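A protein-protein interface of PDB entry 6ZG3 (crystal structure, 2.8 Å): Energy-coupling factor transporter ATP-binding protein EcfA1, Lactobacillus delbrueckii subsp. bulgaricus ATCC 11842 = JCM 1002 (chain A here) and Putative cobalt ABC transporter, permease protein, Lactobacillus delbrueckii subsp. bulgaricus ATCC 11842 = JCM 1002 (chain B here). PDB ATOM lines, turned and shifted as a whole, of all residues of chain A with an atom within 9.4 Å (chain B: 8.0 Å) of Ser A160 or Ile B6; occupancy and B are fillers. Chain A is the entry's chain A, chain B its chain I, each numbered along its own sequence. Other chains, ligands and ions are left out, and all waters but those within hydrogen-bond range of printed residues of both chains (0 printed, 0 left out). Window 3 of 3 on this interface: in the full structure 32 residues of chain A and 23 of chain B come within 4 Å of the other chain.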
ATOM      1  N   ASP A 112     -14.980  14.819 -17.684  1.00  0.00           N
ATOM      2  CA  ASP A 112     -16.150  14.431 -16.917  1.00  0.00           C
ATOM      3  C   ASP A 112     -15.858  13.065 -16.313  1.00  0.00           C
ATOM      4  O   ASP A 112     -14.860  12.425 -16.645  1.00  0.00           O
ATOM      5  CB  ASP A 112     -17.382  14.352 -17.817  1.00  0.00           C
ATOM      6  CG  ASP A 112     -18.227  15.586 -17.757  1.00  0.00           C
ATOM      7  OD1 ASP A 112     -18.214  16.225 -16.695  1.00  0.00           O
ATOM      8  OD2 ASP A 112     -18.916  15.921 -18.738  1.00  0.00           O
ATOM      9  N   PHE A 115     -15.385  14.514 -12.146  1.00  0.00           N
ATOM     10  CA  PHE A 115     -16.033  15.604 -11.429  1.00  0.00           C
ATOM     11  C   PHE A 115     -17.027  15.000 -10.438  1.00  0.00           C
ATOM     12  O   PHE A 115     -18.029  14.403 -10.844  1.00  0.00           O
ATOM     13  CB  PHE A 115     -16.759  16.504 -12.430  1.00  0.00           C
ATOM     14  CG  PHE A 115     -16.622  17.979 -12.174  1.00  0.00           C
ATOM     15  CD1 PHE A 115     -17.191  18.562 -11.058  1.00  0.00           C
ATOM     16  CD2 PHE A 115     -15.976  18.799 -13.100  1.00  0.00           C
ATOM     17  CE1 PHE A 115     -17.089  19.944 -10.854  1.00  0.00           C
ATOM     18  CE2 PHE A 115     -15.869  20.184 -12.899  1.00  0.00           C
ATOM     19  CZ  PHE A 115     -16.417  20.752 -11.781  1.00  0.00           C
ATOM     20  N   GLY A 117     -18.206  17.068  -7.696  1.00  0.00           N
ATOM     21  CA  GLY A 117     -19.042  18.125  -7.170  1.00  0.00           C
ATOM     22  C   GLY A 117     -20.016  18.706  -8.181  1.00  0.00           C
ATOM     23  O   GLY A 117     -19.821  18.661  -9.384  1.00  0.00           O
ATOM     24  N   ALA A 118     -21.094  19.298  -7.674  1.00  0.00           N
ATOM     25  CA  ALA A 118     -22.060  19.911  -8.573  1.00  0.00           C
ATOM     26  C   ALA A 118     -21.555  21.235  -9.124  1.00  0.00           C
ATOM     27  O   ALA A 118     -22.132  21.760 -10.095  1.00  0.00           O
ATOM     28  CB  ALA A 118     -23.404  20.090  -7.852  1.00  0.00           C
ATOM     29  N   THR A 119     -20.494  21.771  -8.516  1.00  0.00           N
ATOM     30  CA  THR A 119     -19.793  22.947  -8.996  1.00  0.00           C
ATOM     31  C   THR A 119     -18.297  22.773  -8.795  1.00  0.00           C
ATOM     32  O   THR A 119     -17.836  21.929  -8.017  1.00  0.00           O
ATOM     33  CB  THR A 119     -20.211  24.190  -8.277  1.00  0.00           C
ATOM     34  OG1 THR A 119     -20.113  23.928  -6.872  1.00  0.00           O
ATOM     35  CG2 THR A 119     -21.609  24.563  -8.668  1.00  0.00           C
ATOM     36  N   VAL A 120     -17.557  23.641  -9.495  1.00  0.00           N
ATOM     37  CA  VAL A 120     -16.097  23.709  -9.417  1.00  0.00           C
ATOM     38  C   VAL A 120     -15.610  23.678  -7.980  1.00  0.00           C
ATOM     39  O   VAL A 120     -14.796  22.827  -7.597  1.00  0.00           O
ATOM     40  CB  VAL A 120     -15.618  24.972 -10.139  1.00  0.00           C
ATOM     41  CG1 VAL A 120     -14.125  25.149  -9.982  1.00  0.00           C
ATOM     42  CG2 VAL A 120     -16.002  24.848 -11.573  1.00  0.00           C
ATOM     43  N   ASP A 156     -18.453  28.952  -9.492  1.00  0.00           N
ATOM     44  CA  ASP A 156     -19.753  28.374  -9.180  1.00  0.00           C
ATOM     45  C   ASP A 156     -20.408  27.713 -10.378  1.00  0.00           C
ATOM     46  O   ASP A 156     -21.614  27.464 -10.351  1.00  0.00           O
ATOM     47  CB  ASP A 156     -20.672  29.454  -8.606  1.00  0.00           C
ATOM     48  CG  ASP A 156     -20.288  29.836  -7.202  1.00  0.00           C
ATOM     49  OD1 ASP A 156     -19.839  28.937  -6.439  1.00  0.00           O
ATOM     50  OD2 ASP A 156     -20.425  31.039  -6.874  1.00  0.00           O
ATOM     51  N   SER A 157     -19.663  27.448 -11.438  1.00  0.00           N
ATOM     52  CA  SER A 157     -20.300  26.891 -12.616  1.00  0.00           C
ATOM     53  C   SER A 157     -20.495  25.390 -12.475  1.00  0.00           C
ATOM     54  O   SER A 157     -19.770  24.703 -11.751  1.00  0.00           O
ATOM     55  CB  SER A 157     -19.490  27.205 -13.859  1.00  0.00           C
ATOM     56  OG  SER A 157     -19.763  28.530 -14.242  1.00  0.00           O
ATOM     57  N   GLU A 158     -21.531  24.897 -13.143  1.00  0.00           N
ATOM     58  CA  GLU A 158     -21.857  23.480 -13.191  1.00  0.00           C
ATOM     59  C   GLU A 158     -21.103  22.803 -14.336  1.00  0.00           C
ATOM     60  O   GLU A 158     -21.041  23.345 -15.462  1.00  0.00           O
ATOM     61  CB  GLU A 158     -23.370  23.275 -13.360  1.00  0.00           C
ATOM     62  CG  GLU A 158     -24.195  23.737 -12.167  1.00  0.00           C
ATOM     63  CD  GLU A 158     -25.695  23.788 -12.456  1.00  0.00           C
ATOM     64  OE1 GLU A 158     -26.351  22.715 -12.425  1.00  0.00           O
ATOM     65  OE2 GLU A 158     -26.218  24.901 -12.708  1.00  0.00           O
ATOM     66  N   PRO A 159     -20.530  21.636 -14.030  1.00  0.00           N
ATOM     67  CA  PRO A 159     -19.741  20.893 -15.022  1.00  0.00           C
ATOM     68  C   PRO A 159     -20.437  20.717 -16.364  1.00  0.00           C
ATOM     69  O   PRO A 159     -19.765  20.660 -17.405  1.00  0.00           O
ATOM     70  CB  PRO A 159     -19.522  19.534 -14.333  1.00  0.00           C
ATOM     71  CG  PRO A 159     -19.640  19.793 -12.939  1.00  0.00           C
ATOM     72  CD  PRO A 159     -20.573  20.945 -12.733  1.00  0.00           C
ATOM     73  N   SER A 160     -21.765  20.601 -16.384  1.00  0.00           N
ATOM     74  CA  SER A 160     -22.430  20.515 -17.671  1.00  0.00           C
ATOM     75  C   SER A 160     -22.244  21.784 -18.497  1.00  0.00           C
ATOM     76  O   SER A 160     -22.570  21.776 -19.685  1.00  0.00           O
ATOM     77  CB  SER A 160     -23.920  20.210 -17.480  1.00  0.00           C
ATOM     78  OG  SER A 160     -24.583  21.138 -16.626  1.00  0.00           O
ATOM     79  N   ASN A 161     -21.735  22.867 -17.909  1.00  0.00           N
ATOM     80  CA  ASN A 161     -21.508  24.104 -18.647  1.00  0.00           C
ATOM     81  C   ASN A 161     -20.033  24.406 -18.845  1.00  0.00           C
ATOM     82  O   ASN A 161     -19.679  25.520 -19.244  1.00  0.00           O
ATOM     83  CB  ASN A 161     -22.191  25.279 -17.953  1.00  0.00           C
ATOM     84  CG  ASN A 161     -23.653  25.022 -17.702  1.00  0.00           C
ATOM     85  OD1 ASN A 161     -24.025  24.614 -16.604  1.00  0.00           O
ATOM     86  ND2 ASN A 161     -24.496  25.253 -18.709  1.00  0.00           N
ATOM     87  N   LEU A 162     -19.169  23.453 -18.551  1.00  0.00           N
ATOM     88  CA  LEU A 162     -17.738  23.642 -18.618  1.00  0.00           C
ATOM     89  C   LEU A 162     -17.176  22.769 -19.707  1.00  0.00           C
ATOM     90  O   LEU A 162     -17.531  21.596 -19.798  1.00  0.00           O
ATOM     91  CB  LEU A 162     -17.066  23.244 -17.316  1.00  0.00           C
ATOM     92  CG  LEU A 162     -16.769  24.273 -16.251  1.00  0.00           C
ATOM     93  CD1 LEU A 162     -17.762  25.390 -16.335  1.00  0.00           C
ATOM     94  CD2 LEU A 162     -16.790  23.551 -14.892  1.00  0.00           C
ATOM     95  N   SER A 163     -16.235  23.318 -20.470  1.00  0.00           N
ATOM     96  CA  SER A 163     -15.515  22.558 -21.472  1.00  0.00           C
ATOM     97  C   SER A 163     -14.670  21.464 -20.798  1.00  0.00           C
ATOM     98  O   SER A 163     -14.539  21.396 -19.573  1.00  0.00           O
ATOM     99  CB  SER A 163     -14.644  23.489 -22.300  1.00  0.00           C
ATOM    100  OG  SER A 163     -13.292  23.406 -21.887  1.00  0.00           O
ATOM    101  N   GLY A 164     -14.142  20.558 -21.620  1.00  0.00           N
ATOM    102  CA  GLY A 164     -13.225  19.554 -21.115  1.00  0.00           C
ATOM    103  C   GLY A 164     -11.903  20.145 -20.677  1.00  0.00           C
ATOM    104  O   GLY A 164     -11.286  19.642 -19.726  1.00  0.00           O
ATOM    105  N   GLN A 166     -11.514  23.075 -19.261  1.00  0.00           N
ATOM    106  CA  GLN A 166     -11.790  23.599 -17.935  1.00  0.00           C
ATOM    107  C   GLN A 166     -11.832  22.472 -16.915  1.00  0.00           C
ATOM    108  O   GLN A 166     -11.134  22.531 -15.903  1.00  0.00           O
ATOM    109  CB  GLN A 166     -13.100  24.376 -17.958  1.00  0.00           C
ATOM    110  CG  GLN A 166     -13.191  25.202 -19.168  1.00  0.00           C
ATOM    111  CD  GLN A 166     -14.241  26.268 -19.077  1.00  0.00           C
ATOM    112  OE1 GLN A 166     -15.375  26.135 -19.546  1.00  0.00           O
ATOM    113  NE2 GLN A 166     -13.865  27.363 -18.463  1.00  0.00           N
ATOM    114  N   LYS A 167     -12.586  21.410 -17.192  1.00  0.00           N
ATOM    115  CA  LYS A 167     -12.718  20.350 -16.202  1.00  0.00           C
ATOM    116  C   LYS A 167     -11.394  19.656 -15.935  1.00  0.00           C
ATOM    117  O   LYS A 167     -11.183  19.153 -14.824  1.00  0.00           O
ATOM    118  CB  LYS A 167     -13.798  19.352 -16.638  1.00  0.00           C
ATOM    119  CG  LYS A 167     -15.161  20.051 -16.825  1.00  0.00           C
ATOM    120  CD  LYS A 167     -16.302  19.074 -16.970  1.00  0.00           C
ATOM    121  CE  LYS A 167     -16.333  18.471 -18.335  1.00  0.00           C
ATOM    122  NZ  LYS A 167     -17.293  19.227 -19.172  1.00  0.00           N
ATOM    123  N   ILE B   6     -31.328  19.970 -13.054  1.00  0.00           N
ATOM    124  CA  ILE B   6     -31.375  21.419 -13.210  1.00  0.00           C
ATOM    125  C   ILE B   6     -32.828  21.865 -13.411  1.00  0.00           C
ATOM    126  O   ILE B   6     -33.345  21.861 -14.534  1.00  0.00           O
ATOM    127  CB  ILE B   6     -30.454  21.892 -14.369  1.00  0.00           C
ATOM    128  CG1 ILE B   6     -28.995  21.641 -14.013  1.00  0.00           C
ATOM    129  CG2 ILE B   6     -30.613  23.373 -14.643  1.00  0.00           C
ATOM    130  CD1 ILE B   6     -28.043  22.153 -15.059  1.00  0.00           C
ATOM    131  N   GLY B   7     -33.491  22.220 -12.306  1.00  0.00           N
ATOM    132  CA  GLY B   7     -34.847  22.743 -12.359  1.00  0.00           C
ATOM    133  C   GLY B   7     -34.973  24.211 -12.734  1.00  0.00           C
ATOM    134  O   GLY B   7     -35.884  24.884 -12.246  1.00  0.00           O
ATOM    135  N   ARG B   8     -34.089  24.717 -13.592  1.00  0.00           N
ATOM    136  CA  ARG B   8     -34.062  26.121 -14.019  1.00  0.00           C
ATOM    137  C   ARG B   8     -34.074  27.082 -12.818  1.00  0.00           C
ATOM    138  O   ARG B   8     -34.988  27.883 -12.615  1.00  0.00           O
ATOM    139  CB  ARG B   8     -35.205  26.419 -15.002  1.00  0.00           C
ATOM    140  CG  ARG B   8     -34.812  26.298 -16.494  1.00  0.00           C
ATOM    141  CD  ARG B   8     -33.302  26.029 -16.696  1.00  0.00           C
ATOM    142  NE  ARG B   8     -32.622  27.026 -17.535  1.00  0.00           N
ATOM    143  CZ  ARG B   8     -32.082  26.777 -18.730  1.00  0.00           C
ATOM    144  NH1 ARG B   8     -31.484  27.752 -19.411  1.00  0.00           N
ATOM    145  NH2 ARG B   8     -32.134  25.554 -19.241  1.00  0.00           N
ATOM    146  N   TYR B   9     -33.022  26.964 -12.002  1.00  0.00           N
ATOM    147  CA  TYR B   9     -32.830  27.818 -10.835  1.00  0.00           C
ATOM    148  C   TYR B   9     -32.171  29.124 -11.275  1.00  0.00           C
ATOM    149  O   TYR B   9     -31.002  29.141 -11.662  1.00  0.00           O
ATOM    150  CB  TYR B   9     -31.984  27.107  -9.784  1.00  0.00           C
ATOM    151  CG  TYR B   9     -31.189  28.054  -8.917  1.00  0.00           C
ATOM    152  CD1 TYR B   9     -31.832  28.994  -8.137  1.00  0.00           C
ATOM    153  CD2 TYR B   9     -29.798  28.009  -8.878  1.00  0.00           C
ATOM    154  CE1 TYR B   9     -31.140  29.864  -7.344  1.00  0.00           C
ATOM    155  CE2 TYR B   9     -29.084  28.891  -8.075  1.00  0.00           C
ATOM    156  CZ  TYR B   9     -29.780  29.815  -7.303  1.00  0.00           C
ATOM    157  OH  TYR B   9     -29.170  30.723  -6.477  1.00  0.00           O
ATOM    158  N   LEU B  10     -32.904  30.180 -11.242  1.00  0.00           N
ATOM    159  CA  LEU B  10     -32.402  31.529 -11.493  1.00  0.00           C
ATOM    160  C   LEU B  10     -31.913  32.165 -10.190  1.00  0.00           C
ATOM    161  O   LEU B  10     -32.627  32.100  -9.184  1.00  0.00           O
ATOM    162  CB  LEU B  10     -33.509  32.381 -12.105  1.00  0.00           C
ATOM    163  CG  LEU B  10     -33.492  33.909 -12.043  1.00  0.00           C
ATOM    164  CD1 LEU B  10     -34.276  34.438 -13.229  1.00  0.00           C
ATOM    165  CD2 LEU B  10     -34.093  34.459 -10.752  1.00  0.00           C
ATOM    166  N   THR B 127     -38.364  25.532  -6.674  1.00  0.00           N
ATOM    167  CA  THR B 127     -37.502  25.084  -7.766  1.00  0.00           C
ATOM    168  C   THR B 127     -36.632  26.210  -8.343  1.00  0.00           C
ATOM    169  O   THR B 127     -35.437  26.013  -8.614  1.00  0.00           O
ATOM    170  CB  THR B 127     -38.410  24.448  -8.813  1.00  0.00           C
ATOM    171  OG1 THR B 127     -38.400  23.025  -8.636  1.00  0.00           O
ATOM    172  CG2 THR B 127     -38.011  24.820 -10.209  1.00  0.00           C
ATOM    173  N   PRO B 132     -30.072  23.504  -6.752  1.00  0.00           N
ATOM    174  CA  PRO B 132     -30.250  22.049  -6.712  1.00  0.00           C
ATOM    175  C   PRO B 132     -29.449  21.353  -5.626  1.00  0.00           C
ATOM    176  O   PRO B 132     -30.000  20.471  -4.960  1.00  0.00           O
ATOM    177  CB  PRO B 132     -29.823  21.639  -8.120  1.00  0.00           C
ATOM    178  CG  PRO B 132     -30.325  22.800  -8.953  1.00  0.00           C
ATOM    179  CD  PRO B 132     -30.122  24.029  -8.125  1.00  0.00           C
ATOM    180  N   ALA B 163     -25.906  12.312  -8.568  1.00  0.00           N
ATOM    181  CA  ALA B 163     -26.999  12.117  -9.504  1.00  0.00           C
ATOM    182  C   ALA B 163     -27.427  13.436 -10.123  1.00  0.00           C
ATOM    183  O   ALA B 163     -27.539  13.554 -11.347  1.00  0.00           O
ATOM    184  CB  ALA B 163     -28.175  11.437  -8.791  1.00  0.00           C
ATOM    185  N   LEU B 164     -27.714  14.431  -9.290  1.00  0.00           N
ATOM    186  CA  LEU B 164     -28.184  15.696  -9.832  1.00  0.00           C
ATOM    187  C   LEU B 164     -27.121  16.346 -10.710  1.00  0.00           C
ATOM    188  O   LEU B 164     -27.462  17.130 -11.614  1.00  0.00           O
ATOM    189  CB  LEU B 164     -28.585  16.635  -8.685  1.00  0.00           C
ATOM    190  CG  LEU B 164     -29.851  16.250  -7.930  1.00  0.00           C
ATOM    191  CD1 LEU B 164     -29.967  17.107  -6.691  1.00  0.00           C
ATOM    192  CD2 LEU B 164     -31.093  16.399  -8.833  1.00  0.00           C
ATOM    193  N   ARG B 165     -25.845  16.026 -10.456  1.00  0.00           N
ATOM    194  CA  ARG B 165     -24.742  16.618 -11.194  1.00  0.00           C
ATOM    195  C   ARG B 165     -24.594  16.002 -12.585  1.00  0.00           C
ATOM    196  O   ARG B 165     -24.215  16.694 -13.547  1.00  0.00           O
ATOM    197  CB  ARG B 165     -23.465  16.425 -10.368  1.00  0.00           C
ATOM    198  CG  ARG B 165     -22.162  16.816 -11.047  1.00  0.00           C
ATOM    199  CD  ARG B 165     -21.425  15.655 -11.646  1.00  0.00           C
ATOM    200  NE  ARG B 165     -21.460  15.816 -13.090  1.00  0.00           N
ATOM    201  CZ  ARG B 165     -20.518  15.372 -13.901  1.00  0.00           C
ATOM    202  NH1 ARG B 165     -19.468  14.727 -13.400  1.00  0.00           N
ATOM    203  NH2 ARG B 165     -20.628  15.575 -15.209  1.00  0.00           N
ATOM    204  N   PHE B 166     -24.904  14.705 -12.698  1.00  0.00           N
ATOM    205  CA  PHE B 166     -24.873  13.946 -13.950  1.00  0.00           C
ATOM    206  C   PHE B 166     -26.197  13.946 -14.720  1.00  0.00           C
ATOM    207  O   PHE B 166     -26.232  13.466 -15.859  1.00  0.00           O
ATOM    208  CB  PHE B 166     -24.507  12.494 -13.664  1.00  0.00           C
ATOM    209  CG  PHE B 166     -23.046  12.221 -13.658  1.00  0.00           C
ATOM    210  CD1 PHE B 166     -22.352  12.049 -14.859  1.00  0.00           C
ATOM    211  CD2 PHE B 166     -22.355  12.126 -12.446  1.00  0.00           C
ATOM    212  CE1 PHE B 166     -20.991  11.780 -14.858  1.00  0.00           C
ATOM    213  CE2 PHE B 166     -20.996  11.846 -12.426  1.00  0.00           C
ATOM    214  CZ  PHE B 166     -20.308  11.677 -13.634  1.00  0.00           C
ATOM    215  N   VAL B 167     -27.287  14.398 -14.113  1.00  0.00           N
ATOM    216  CA  VAL B 167     -28.579  14.402 -14.801  1.00  0.00           C
ATOM    217  C   VAL B 167     -28.459  15.166 -16.124  1.00  0.00           C
ATOM    218  O   VAL B 167     -28.972  14.705 -17.147  1.00  0.00           O
ATOM    219  CB  VAL B 167     -29.703  14.934 -13.878  1.00  0.00           C
ATOM    220  CG1 VAL B 167     -30.846  15.556 -14.662  1.00  0.00           C
ATOM    221  CG2 VAL B 167     -30.229  13.803 -13.035  1.00  0.00           C
ATOM    222  N   PRO B 168     -27.789  16.284 -16.195  1.00  0.00           N
ATOM    223  CA  PRO B 168     -27.737  16.966 -17.496  1.00  0.00           C
ATOM    224  C   PRO B 168     -26.674  16.366 -18.425  1.00  0.00           C
ATOM    225  O   PRO B 168     -26.818  16.368 -19.655  1.00  0.00           O
ATOM    226  CB  PRO B 168     -27.437  18.411 -17.107  1.00  0.00           C
ATOM    227  CG  PRO B 168     -26.688  18.282 -15.809  1.00  0.00           C
ATOM    228  CD  PRO B 168     -27.084  17.041 -15.141  1.00  0.00           C
ATOM    229  N   THR B 169     -25.604  15.832 -17.826  1.00  0.00           N
ATOM    230  CA  THR B 169     -24.566  15.164 -18.602  1.00  0.00           C
ATOM    231  C   THR B 169     -25.123  13.912 -19.286  1.00  0.00           C
ATOM    232  O   THR B 169     -24.984  13.742 -20.512  1.00  0.00           O
ATOM    233  CB  THR B 169     -23.359  14.828 -17.688  1.00  0.00           C
ATOM    234  OG1 THR B 169     -22.453  15.948 -17.600  1.00  0.00           O
ATOM    235  CG2 THR B 169     -22.592  13.618 -18.184  1.00  0.00           C
ATOM    236  N   LEU B 170     -25.826  13.053 -18.520  1.00  0.00           N
ATOM    237  CA  LEU B 170     -26.402  11.858 -19.119  1.00  0.00           C
ATOM    238  C   LEU B 170     -27.510  12.208 -20.079  1.00  0.00           C
ATOM    239  O   LEU B 170     -27.770  11.451 -21.011  1.00  0.00           O
ATOM    240  CB  LEU B 170     -26.908  10.875 -18.075  1.00  0.00           C
ATOM    241  CG  LEU B 170     -25.804  10.171 -17.303  1.00  0.00           C
ATOM    242  CD1 LEU B 170     -26.344   9.158 -16.272  1.00  0.00           C
ATOM    243  CD2 LEU B 170     -24.880   9.502 -18.257  1.00  0.00           C
ATOM    244  N   ASP B 172     -27.453  14.860 -22.164  1.00  0.00           N
ATOM    245  CA  ASP B 172     -26.811  15.166 -23.431  1.00  0.00           C
ATOM    246  C   ASP B 172     -26.347  13.889 -24.104  1.00  0.00           C
ATOM    247  O   ASP B 172     -26.608  13.683 -25.296  1.00  0.00           O
ATOM    248  CB  ASP B 172     -25.655  16.142 -23.247  1.00  0.00           C
ATOM    249  CG  ASP B 172     -26.111  17.494 -22.711  1.00  0.00           C
ATOM    250  OD1 ASP B 172     -27.218  17.580 -22.119  1.00  0.00           O
ATOM    251  OD2 ASP B 172     -25.367  18.481 -22.902  1.00  0.00           O
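The side-chain carboxylate of Asp A112 is in salt-bridge range of the guanidinium group of Arg B165, at 2.9 Å. O of Phe A115 is in hydrogen-bond range of NH1 of Arg B165.
The side-chain carboxylate of Asp A112 lies within salt-bridge range of the side-chain amino group of Lys A167, at 3.7 Å. O of Glu A158 sits close to OD1 of Asn A161, at 3.4 Å. The side-chain hydroxyl of Thr B169 sits at hydrogen-bond distance from the guanidinium group of Arg B165.
Among the printed residues, pairs that only touch across the chains: Asp A112 with Thr B169 (3.7 Å), Gly A117 with Arg B165 (3.4 Å), Ala A118 with Arg B165 (3.96 Å), Glu A158 with Ile B6 (3.2 Å), Ser A160 with Ile B6 (3.9 Å) and Ser A160 with Pro B168 (3.6 Å).
Of the printed residues of chain B, Asp A112 touches Arg B165 and Thr B169. Of the printed residues of chain B, Glu A158 touches Ile B6 (3.2 Å). Ser A160 touches two residues of chain B. Asn A161 touches none of the printed residues of chain B. No residue of chain A comes within 4 Å of Gly B7. Printed residues of chain A within 4 Å of Arg B165: Asp A112 (2.9 Å), Phe A115 (3.0 Å), Gly A117 (3.4 Å) and Ala A118 (3.96 Å). Asp B172 touches none of the printed residues of chain A. The nearest residue of chain B that does not touch Ser A160 is Thr B169 (4.5 Å). The nearest residue of chain A that does not touch Ile B6 is Asn A161 (5.0 Å).
Hydrophobic or aromatic side chains of chain B within 4 Å of the printed part of chain A: Ile B6 and Pro B168. Among the printed residues, 8 pairs touch across the chains.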
